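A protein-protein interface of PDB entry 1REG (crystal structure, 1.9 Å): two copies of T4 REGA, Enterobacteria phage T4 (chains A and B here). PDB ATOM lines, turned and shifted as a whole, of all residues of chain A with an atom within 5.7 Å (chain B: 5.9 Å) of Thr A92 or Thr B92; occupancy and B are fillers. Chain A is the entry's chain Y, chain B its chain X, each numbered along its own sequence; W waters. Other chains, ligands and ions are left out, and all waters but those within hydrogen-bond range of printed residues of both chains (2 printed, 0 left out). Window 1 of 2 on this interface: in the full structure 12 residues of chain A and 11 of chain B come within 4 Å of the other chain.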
ATOM      1  N   ILE A   2      28.749  10.659  36.153  1.00  0.00           N
ATOM      2  CA  ILE A   2      27.909  10.872  34.956  1.00  0.00           C
ATOM      3  C   ILE A   2      27.646  12.342  34.931  1.00  0.00           C
ATOM      4  O   ILE A   2      27.301  12.866  35.978  1.00  0.00           O
ATOM      5  CB  ILE A   2      26.596  10.042  35.082  1.00  0.00           C
ATOM      6  CG1 ILE A   2      26.960   8.599  34.888  1.00  0.00           C
ATOM      7  CG2 ILE A   2      25.562  10.394  34.038  1.00  0.00           C
ATOM      8  CD1 ILE A   2      26.114   7.736  35.847  1.00  0.00           C
ATOM      9  N   ASP A  72      24.500   3.904  37.299  1.00  0.00           N
ATOM     10  CA  ASP A  72      23.914   4.201  36.019  1.00  0.00           C
ATOM     11  C   ASP A  72      22.408   4.014  36.033  1.00  0.00           C
ATOM     12  O   ASP A  72      21.698   4.862  35.483  1.00  0.00           O
ATOM     13  CB  ASP A  72      24.582   3.319  34.993  1.00  0.00           C
ATOM     14  CG  ASP A  72      26.049   3.693  34.754  1.00  0.00           C
ATOM     15  OD1 ASP A  72      26.589   4.554  35.435  1.00  0.00           O
ATOM     16  OD2 ASP A  72      26.687   3.119  33.876  1.00  0.00           O
ATOM     17  N   TRP A  76      19.759   6.955  35.361  1.00  0.00           N
ATOM     18  CA  TRP A  76      18.676   6.806  34.424  1.00  0.00           C
ATOM     19  C   TRP A  76      17.289   6.865  35.049  1.00  0.00           C
ATOM     20  O   TRP A  76      16.361   7.348  34.413  1.00  0.00           O
ATOM     21  CB  TRP A  76      18.825   5.518  33.705  1.00  0.00           C
ATOM     22  CG  TRP A  76      19.806   5.670  32.582  1.00  0.00           C
ATOM     23  CD1 TRP A  76      21.006   5.026  32.574  1.00  0.00           C
ATOM     24  CD2 TRP A  76      19.610   6.463  31.506  1.00  0.00           C
ATOM     25  NE1 TRP A  76      21.595   5.424  31.485  1.00  0.00           N
ATOM     26  CE2 TRP A  76      20.797   6.275  30.825  1.00  0.00           C
ATOM     27  CE3 TRP A  76      18.639   7.295  31.028  1.00  0.00           C
ATOM     28  CZ2 TRP A  76      21.027   6.930  29.640  1.00  0.00           C
ATOM     29  CZ3 TRP A  76      18.872   7.944  29.845  1.00  0.00           C
ATOM     30  CH2 TRP A  76      20.047   7.762  29.166  1.00  0.00           C
ATOM     31  N   ILE A  86      20.895  13.403  31.303  1.00  0.00           N
ATOM     32  CA  ILE A  86      22.241  12.868  31.287  1.00  0.00           C
ATOM     33  C   ILE A  86      22.750  13.540  30.032  1.00  0.00           C
ATOM     34  O   ILE A  86      22.072  13.568  29.009  1.00  0.00           O
ATOM     35  CB  ILE A  86      22.184  11.339  31.195  1.00  0.00           C
ATOM     36  CG1 ILE A  86      21.492  10.887  32.479  1.00  0.00           C
ATOM     37  CG2 ILE A  86      23.541  10.697  30.995  1.00  0.00           C
ATOM     38  CD1 ILE A  86      21.306   9.392  32.613  1.00  0.00           C
ATOM     39  N   GLN A  90      27.668   9.757  26.579  1.00  0.00           N
ATOM     40  CA  GLN A  90      28.492   9.052  27.550  1.00  0.00           C
ATOM     41  C   GLN A  90      28.102   7.606  27.400  1.00  0.00           C
ATOM     42  O   GLN A  90      26.993   7.343  26.967  1.00  0.00           O
ATOM     43  CB  GLN A  90      28.199   9.466  28.970  1.00  0.00           C
ATOM     44  CG  GLN A  90      28.476  10.922  29.214  1.00  0.00           C
ATOM     45  CD  GLN A  90      27.818  11.416  30.481  1.00  0.00           C
ATOM     46  OE1 GLN A  90      28.493  11.694  31.461  1.00  0.00           O
ATOM     47  NE2 GLN A  90      26.527  11.615  30.555  1.00  0.00           N
ATOM     48  N   ARG A  91      28.957   6.668  27.723  1.00  0.00           N
ATOM     49  CA  ARG A  91      28.694   5.249  27.608  1.00  0.00           C
ATOM     50  C   ARG A  91      28.249   4.692  28.941  1.00  0.00           C
ATOM     51  O   ARG A  91      29.046   4.545  29.869  1.00  0.00           O
ATOM     52  CB  ARG A  91      29.964   4.568  27.140  1.00  0.00           C
ATOM     53  CG  ARG A  91      29.692   3.196  26.601  1.00  0.00           C
ATOM     54  CD  ARG A  91      30.792   2.885  25.583  1.00  0.00           C
ATOM     55  NE  ARG A  91      32.061   2.434  26.137  1.00  0.00           N
ATOM     56  CZ  ARG A  91      32.111   1.255  26.780  1.00  0.00           C
ATOM     57  NH1 ARG A  91      31.020   0.488  26.903  1.00  0.00           N
ATOM     58  NH2 ARG A  91      33.244   0.839  27.387  1.00  0.00           N
ATOM     59  N   THR A  92      26.994   4.313  29.089  1.00  0.00           N
ATOM     60  CA  THR A  92      26.535   3.872  30.390  1.00  0.00           C
ATOM     61  C   THR A  92      25.727   2.573  30.302  1.00  0.00           C
ATOM     62  O   THR A  92      25.412   2.063  29.231  1.00  0.00           O
ATOM     63  CB  THR A  92      25.716   5.062  31.041  1.00  0.00           C
ATOM     64  OG1 THR A  92      24.459   5.113  30.386  1.00  0.00           O
ATOM     65  CG2 THR A  92      26.338   6.453  30.879  1.00  0.00           C
ATOM     66  N   PHE A  93      25.463   1.937  31.437  1.00  0.00           N
ATOM     67  CA  PHE A  93      24.600   0.767  31.461  1.00  0.00           C
ATOM     68  C   PHE A  93      23.224   1.415  31.367  1.00  0.00           C
ATOM     69  O   PHE A  93      22.923   2.228  32.229  1.00  0.00           O
ATOM     70  CB  PHE A  93      24.766   0.001  32.789  1.00  0.00           C
ATOM     71  CG  PHE A  93      26.121  -0.711  32.989  1.00  0.00           C
ATOM     72  CD1 PHE A  93      26.315  -1.992  32.476  1.00  0.00           C
ATOM     73  CD2 PHE A  93      27.161  -0.114  33.710  1.00  0.00           C
ATOM     74  CE1 PHE A  93      27.516  -2.659  32.678  1.00  0.00           C
ATOM     75  CE2 PHE A  93      28.365  -0.809  33.904  1.00  0.00           C
ATOM     76  CZ  PHE A  93      28.543  -2.078  33.385  1.00  0.00           C
ATOM     77  N   MET A  94      22.497   1.258  30.281  1.00  0.00           N
ATOM     78  CA  MET A  94      21.181   1.829  30.058  1.00  0.00           C
ATOM     79  C   MET A  94      20.135   0.754  30.267  1.00  0.00           C
ATOM     80  O   MET A  94      18.937   1.054  30.203  1.00  0.00           O
ATOM     81  CB  MET A  94      21.070   2.371  28.617  1.00  0.00           C
ATOM     82  CG  MET A  94      22.207   3.309  28.276  1.00  0.00           C
ATOM     83  SD  MET A  94      22.308   3.757  26.522  1.00  0.00           S
ATOM     84  CE  MET A  94      20.771   4.550  26.243  1.00  0.00           C
ATOM     85  N   ILE B   2      28.116  -5.960  20.830  1.00  0.00           N
ATOM     86  CA  ILE B   2      26.964  -5.901  21.725  1.00  0.00           C
ATOM     87  C   ILE B   2      26.118  -7.178  21.676  1.00  0.00           C
ATOM     88  O   ILE B   2      25.616  -7.520  20.606  1.00  0.00           O
ATOM     89  CB  ILE B   2      26.153  -4.616  21.321  1.00  0.00           C
ATOM     90  CG1 ILE B   2      26.975  -3.326  21.397  1.00  0.00           C
ATOM     91  CG2 ILE B   2      24.959  -4.531  22.239  1.00  0.00           C
ATOM     92  CD1 ILE B   2      27.585  -3.011  22.781  1.00  0.00           C
ATOM     93  N   ASP B  72      26.563   1.182  18.342  1.00  0.00           N
ATOM     94  CA  ASP B  72      25.525   1.153  19.365  1.00  0.00           C
ATOM     95  C   ASP B  72      24.243   1.760  18.899  1.00  0.00           C
ATOM     96  O   ASP B  72      23.203   1.203  19.232  1.00  0.00           O
ATOM     97  CB  ASP B  72      25.953   1.898  20.617  1.00  0.00           C
ATOM     98  CG  ASP B  72      27.171   1.308  21.284  1.00  0.00           C
ATOM     99  OD1 ASP B  72      27.643   0.245  20.913  1.00  0.00           O
ATOM    100  OD2 ASP B  72      27.669   1.934  22.196  1.00  0.00           O
ATOM    101  N   TRP B  76      20.663   0.224  18.820  1.00  0.00           N
ATOM    102  CA  TRP B  76      19.465   0.899  19.268  1.00  0.00           C
ATOM    103  C   TRP B  76      18.386   0.978  18.229  1.00  0.00           C
ATOM    104  O   TRP B  76      17.263   0.623  18.583  1.00  0.00           O
ATOM    105  CB  TRP B  76      19.752   2.313  19.728  1.00  0.00           C
ATOM    106  CG  TRP B  76      20.407   2.319  21.109  1.00  0.00           C
ATOM    107  CD1 TRP B  76      21.659   2.869  21.334  1.00  0.00           C
ATOM    108  CD2 TRP B  76      19.872   1.709  22.210  1.00  0.00           C
ATOM    109  NE1 TRP B  76      21.911   2.571  22.570  1.00  0.00           N
ATOM    110  CE2 TRP B  76      20.889   1.889  23.124  1.00  0.00           C
ATOM    111  CE3 TRP B  76      18.712   1.047  22.551  1.00  0.00           C
ATOM    112  CZ2 TRP B  76      20.757   1.394  24.405  1.00  0.00           C
ATOM    113  CZ3 TRP B  76      18.585   0.561  23.835  1.00  0.00           C
ATOM    114  CH2 TRP B  76      19.602   0.733  24.759  1.00  0.00           C
ATOM    115  N   ILE B  86      18.686  -5.412  22.952  1.00  0.00           N
ATOM    116  CA  ILE B  86      20.057  -5.457  23.468  1.00  0.00           C
ATOM    117  C   ILE B  86      20.044  -6.099  24.864  1.00  0.00           C
ATOM    118  O   ILE B  86      19.103  -5.884  25.635  1.00  0.00           O
ATOM    119  CB  ILE B  86      20.588  -4.013  23.467  1.00  0.00           C
ATOM    120  CG1 ILE B  86      20.562  -3.483  22.056  1.00  0.00           C
ATOM    121  CG2 ILE B  86      22.026  -3.947  23.943  1.00  0.00           C
ATOM    122  CD1 ILE B  86      20.961  -2.004  22.066  1.00  0.00           C
ATOM    123  N   GLN B  90      24.937  -4.209  29.816  1.00  0.00           N
ATOM    124  CA  GLN B  90      26.006  -3.789  28.949  1.00  0.00           C
ATOM    125  C   GLN B  90      26.019  -2.282  28.840  1.00  0.00           C
ATOM    126  O   GLN B  90      24.987  -1.617  28.823  1.00  0.00           O
ATOM    127  CB  GLN B  90      25.835  -4.300  27.582  1.00  0.00           C
ATOM    128  CG  GLN B  90      25.614  -5.754  27.597  1.00  0.00           C
ATOM    129  CD  GLN B  90      25.680  -6.233  26.192  1.00  0.00           C
ATOM    130  OE1 GLN B  90      24.698  -6.521  25.505  1.00  0.00           O
ATOM    131  NE2 GLN B  90      26.919  -6.277  25.728  1.00  0.00           N
ATOM    132  N   ARG B  91      27.237  -1.741  28.855  1.00  0.00           N
ATOM    133  CA  ARG B  91      27.493  -0.333  28.641  1.00  0.00           C
ATOM    134  C   ARG B  91      27.434   0.023  27.182  1.00  0.00           C
ATOM    135  O   ARG B  91      28.124  -0.565  26.347  1.00  0.00           O
ATOM    136  CB  ARG B  91      28.866   0.108  29.115  1.00  0.00           C
ATOM    137  CG  ARG B  91      28.936   0.271  30.611  1.00  0.00           C
ATOM    138  CD  ARG B  91      30.309   0.663  31.061  1.00  0.00           C
ATOM    139  NE  ARG B  91      30.747   1.768  30.242  1.00  0.00           N
ATOM    140  CZ  ARG B  91      31.814   2.489  30.544  1.00  0.00           C
ATOM    141  NH1 ARG B  91      32.555   2.237  31.636  1.00  0.00           N
ATOM    142  NH2 ARG B  91      32.147   3.503  29.747  1.00  0.00           N
ATOM    143  N   THR B  92      26.488   0.919  26.920  1.00  0.00           N
ATOM    144  CA  THR B  92      26.348   1.447  25.586  1.00  0.00           C
ATOM    145  C   THR B  92      26.226   2.949  25.522  1.00  0.00           C
ATOM    146  O   THR B  92      25.884   3.645  26.463  1.00  0.00           O
ATOM    147  CB  THR B  92      25.095   0.806  24.851  1.00  0.00           C
ATOM    148  OG1 THR B  92      24.004   0.917  25.727  1.00  0.00           O
ATOM    149  CG2 THR B  92      25.263  -0.648  24.442  1.00  0.00           C
ATOM    150  N   PHE B  93      26.626   3.485  24.393  1.00  0.00           N
ATOM    151  CA  PHE B  93      26.321   4.847  24.039  1.00  0.00           C
ATOM    152  C   PHE B  93      24.848   5.027  23.703  1.00  0.00           C
ATOM    153  O   PHE B  93      24.117   4.106  23.309  1.00  0.00           O
ATOM    154  CB  PHE B  93      27.114   5.284  22.813  1.00  0.00           C
ATOM    155  CG  PHE B  93      28.585   5.553  23.115  1.00  0.00           C
ATOM    156  CD1 PHE B  93      28.930   6.572  23.996  1.00  0.00           C
ATOM    157  CD2 PHE B  93      29.562   4.803  22.500  1.00  0.00           C
ATOM    158  CE1 PHE B  93      30.238   6.844  24.270  1.00  0.00           C
ATOM    159  CE2 PHE B  93      30.877   5.095  22.787  1.00  0.00           C
ATOM    160  CZ  PHE B  93      31.204   6.104  23.665  1.00  0.00           C
ATOM    161  N   MET B  94      24.427   6.271  23.742  1.00  0.00           N
ATOM    162  CA  MET B  94      23.083   6.636  23.431  1.00  0.00           C
ATOM    163  C   MET B  94      22.990   6.570  21.914  1.00  0.00           C
ATOM    164  O   MET B  94      23.991   6.568  21.179  1.00  0.00           O
ATOM    165  CB  MET B  94      22.842   8.023  23.907  1.00  0.00           C
ATOM    166  CG  MET B  94      23.320   8.241  25.319  1.00  0.00           C
ATOM    167  SD  MET B  94      22.903   9.947  25.732  1.00  0.00           S
ATOM    168  CE  MET B  94      21.940   9.495  27.134  1.00  0.00           C
HETATM  169  O   HOH W   1      35.042   3.336  28.594  1.00  0.00           O
HETATM  170  O   HOH W   2      22.823   0.034  27.834  1.00  0.00           O
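The guanidinium group (NH1) of Arg A91 lies close to the backbone carbonyl oxygen (O) of Arg B91. The backbone NH (N) of Thr B92 is in hydrogen-bond range of the backbone carbonyl oxygen (O) of Thr A92 (2.8 Å). The side-chain hydroxyl of Thr B92 lies within hydrogen-bond range of the side-chain sulfur of Met A94, at 3.4 Å. SD of Met A94 sits close to O of Phe B93, at 3.7 Å.
The side-chain carboxylate (OD2) of Asp B72 lies within hydrogen-bond range of the backbone NH (N) of Phe B93 (2.9 Å). The indole nitrogen (NE1) of Trp B76 is in hydrogen-bond range of the backbone carbonyl oxygen (O) of Phe B93. The backbone NH of Phe A93 is in hydrogen-bond range of the side-chain carboxylate of Asp A72, at 3.0 Å. The indole nitrogen of Trp A76 lies within hydrogen-bond range of the side-chain hydroxyl of Thr A92, 3.1 Å away.
Among the printed residues, pairs that only touch across the chains: Thr A92 with Arg B91, Trp A76 with Met B94, Arg A91 with Thr B92, Phe A93 with Arg B91, Met A94 with Trp B76, Arg A91 with Phe B93, Phe A93 with Gln B90, Gln A90 with Phe B93, Thr A92 with Gln B90 and Gln A90 with Thr B92.
Printed residues of chain B within 4 Å of Thr A92: Gln B90, Arg B91 and Thr B92. Printed residues of chain A within 4 Å of Phe B93: Gln A90, Arg A91 and Met A94. Of the printed residues of chain B, Met A94 touches Trp B76 (3.5 Å), Thr B92 (3.4 Å) and Phe B93 (3.7 Å). Ile B2 touches none of the printed residues of chain A. Asp B72 touches none of the printed residues of chain A. The nearest residue of chain A that does not touch Thr B92 is Phe A93 (4.7 Å).
Hydrophobic or aromatic side chains of chain A within 4 Å of the printed part of chain B: Trp A76, Phe A93 and Met A94. Of the 9 printed residues of chain B, 6 touch a printed residue of chain A. Printed residues of chain B that touch a printed residue of chain A: Trp B76, Gln B90, Arg B91, Thr B92, Phe B93 and Met B94. Among the printed residues, no Asp or Glu carboxylate lies within 4 Å of a Lys or Arg side-chain nitrogen of the other chain.
Gln A90 touches Phe B93, and with the chains exchanged Phe A93 touches Gln B90. Arg A91 touches its own counterpart, Arg B91. Arg A91 touches Thr B92, and with the chains exchanged Thr A92 touches Arg B91. Met A94 touches Phe B93, but with the chains exchanged Phe A93 does not touch Met B94 (8.9 Å). Of the 14 pairs that touch across the chains among the printed residues, 12 have their exchanged pair printed and touching as well.
Water W2 lies within hydrogen-bond range of OG1 of Thr B92 (2.6 Å), N of Met A94 (2.8 Å) and O of Gln B90 (2.9 Å). Water W1 lies within hydrogen-bond range of NH2 of Arg B91 (3.1 Å) and NH2 of Arg A91 (3.3 Å).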
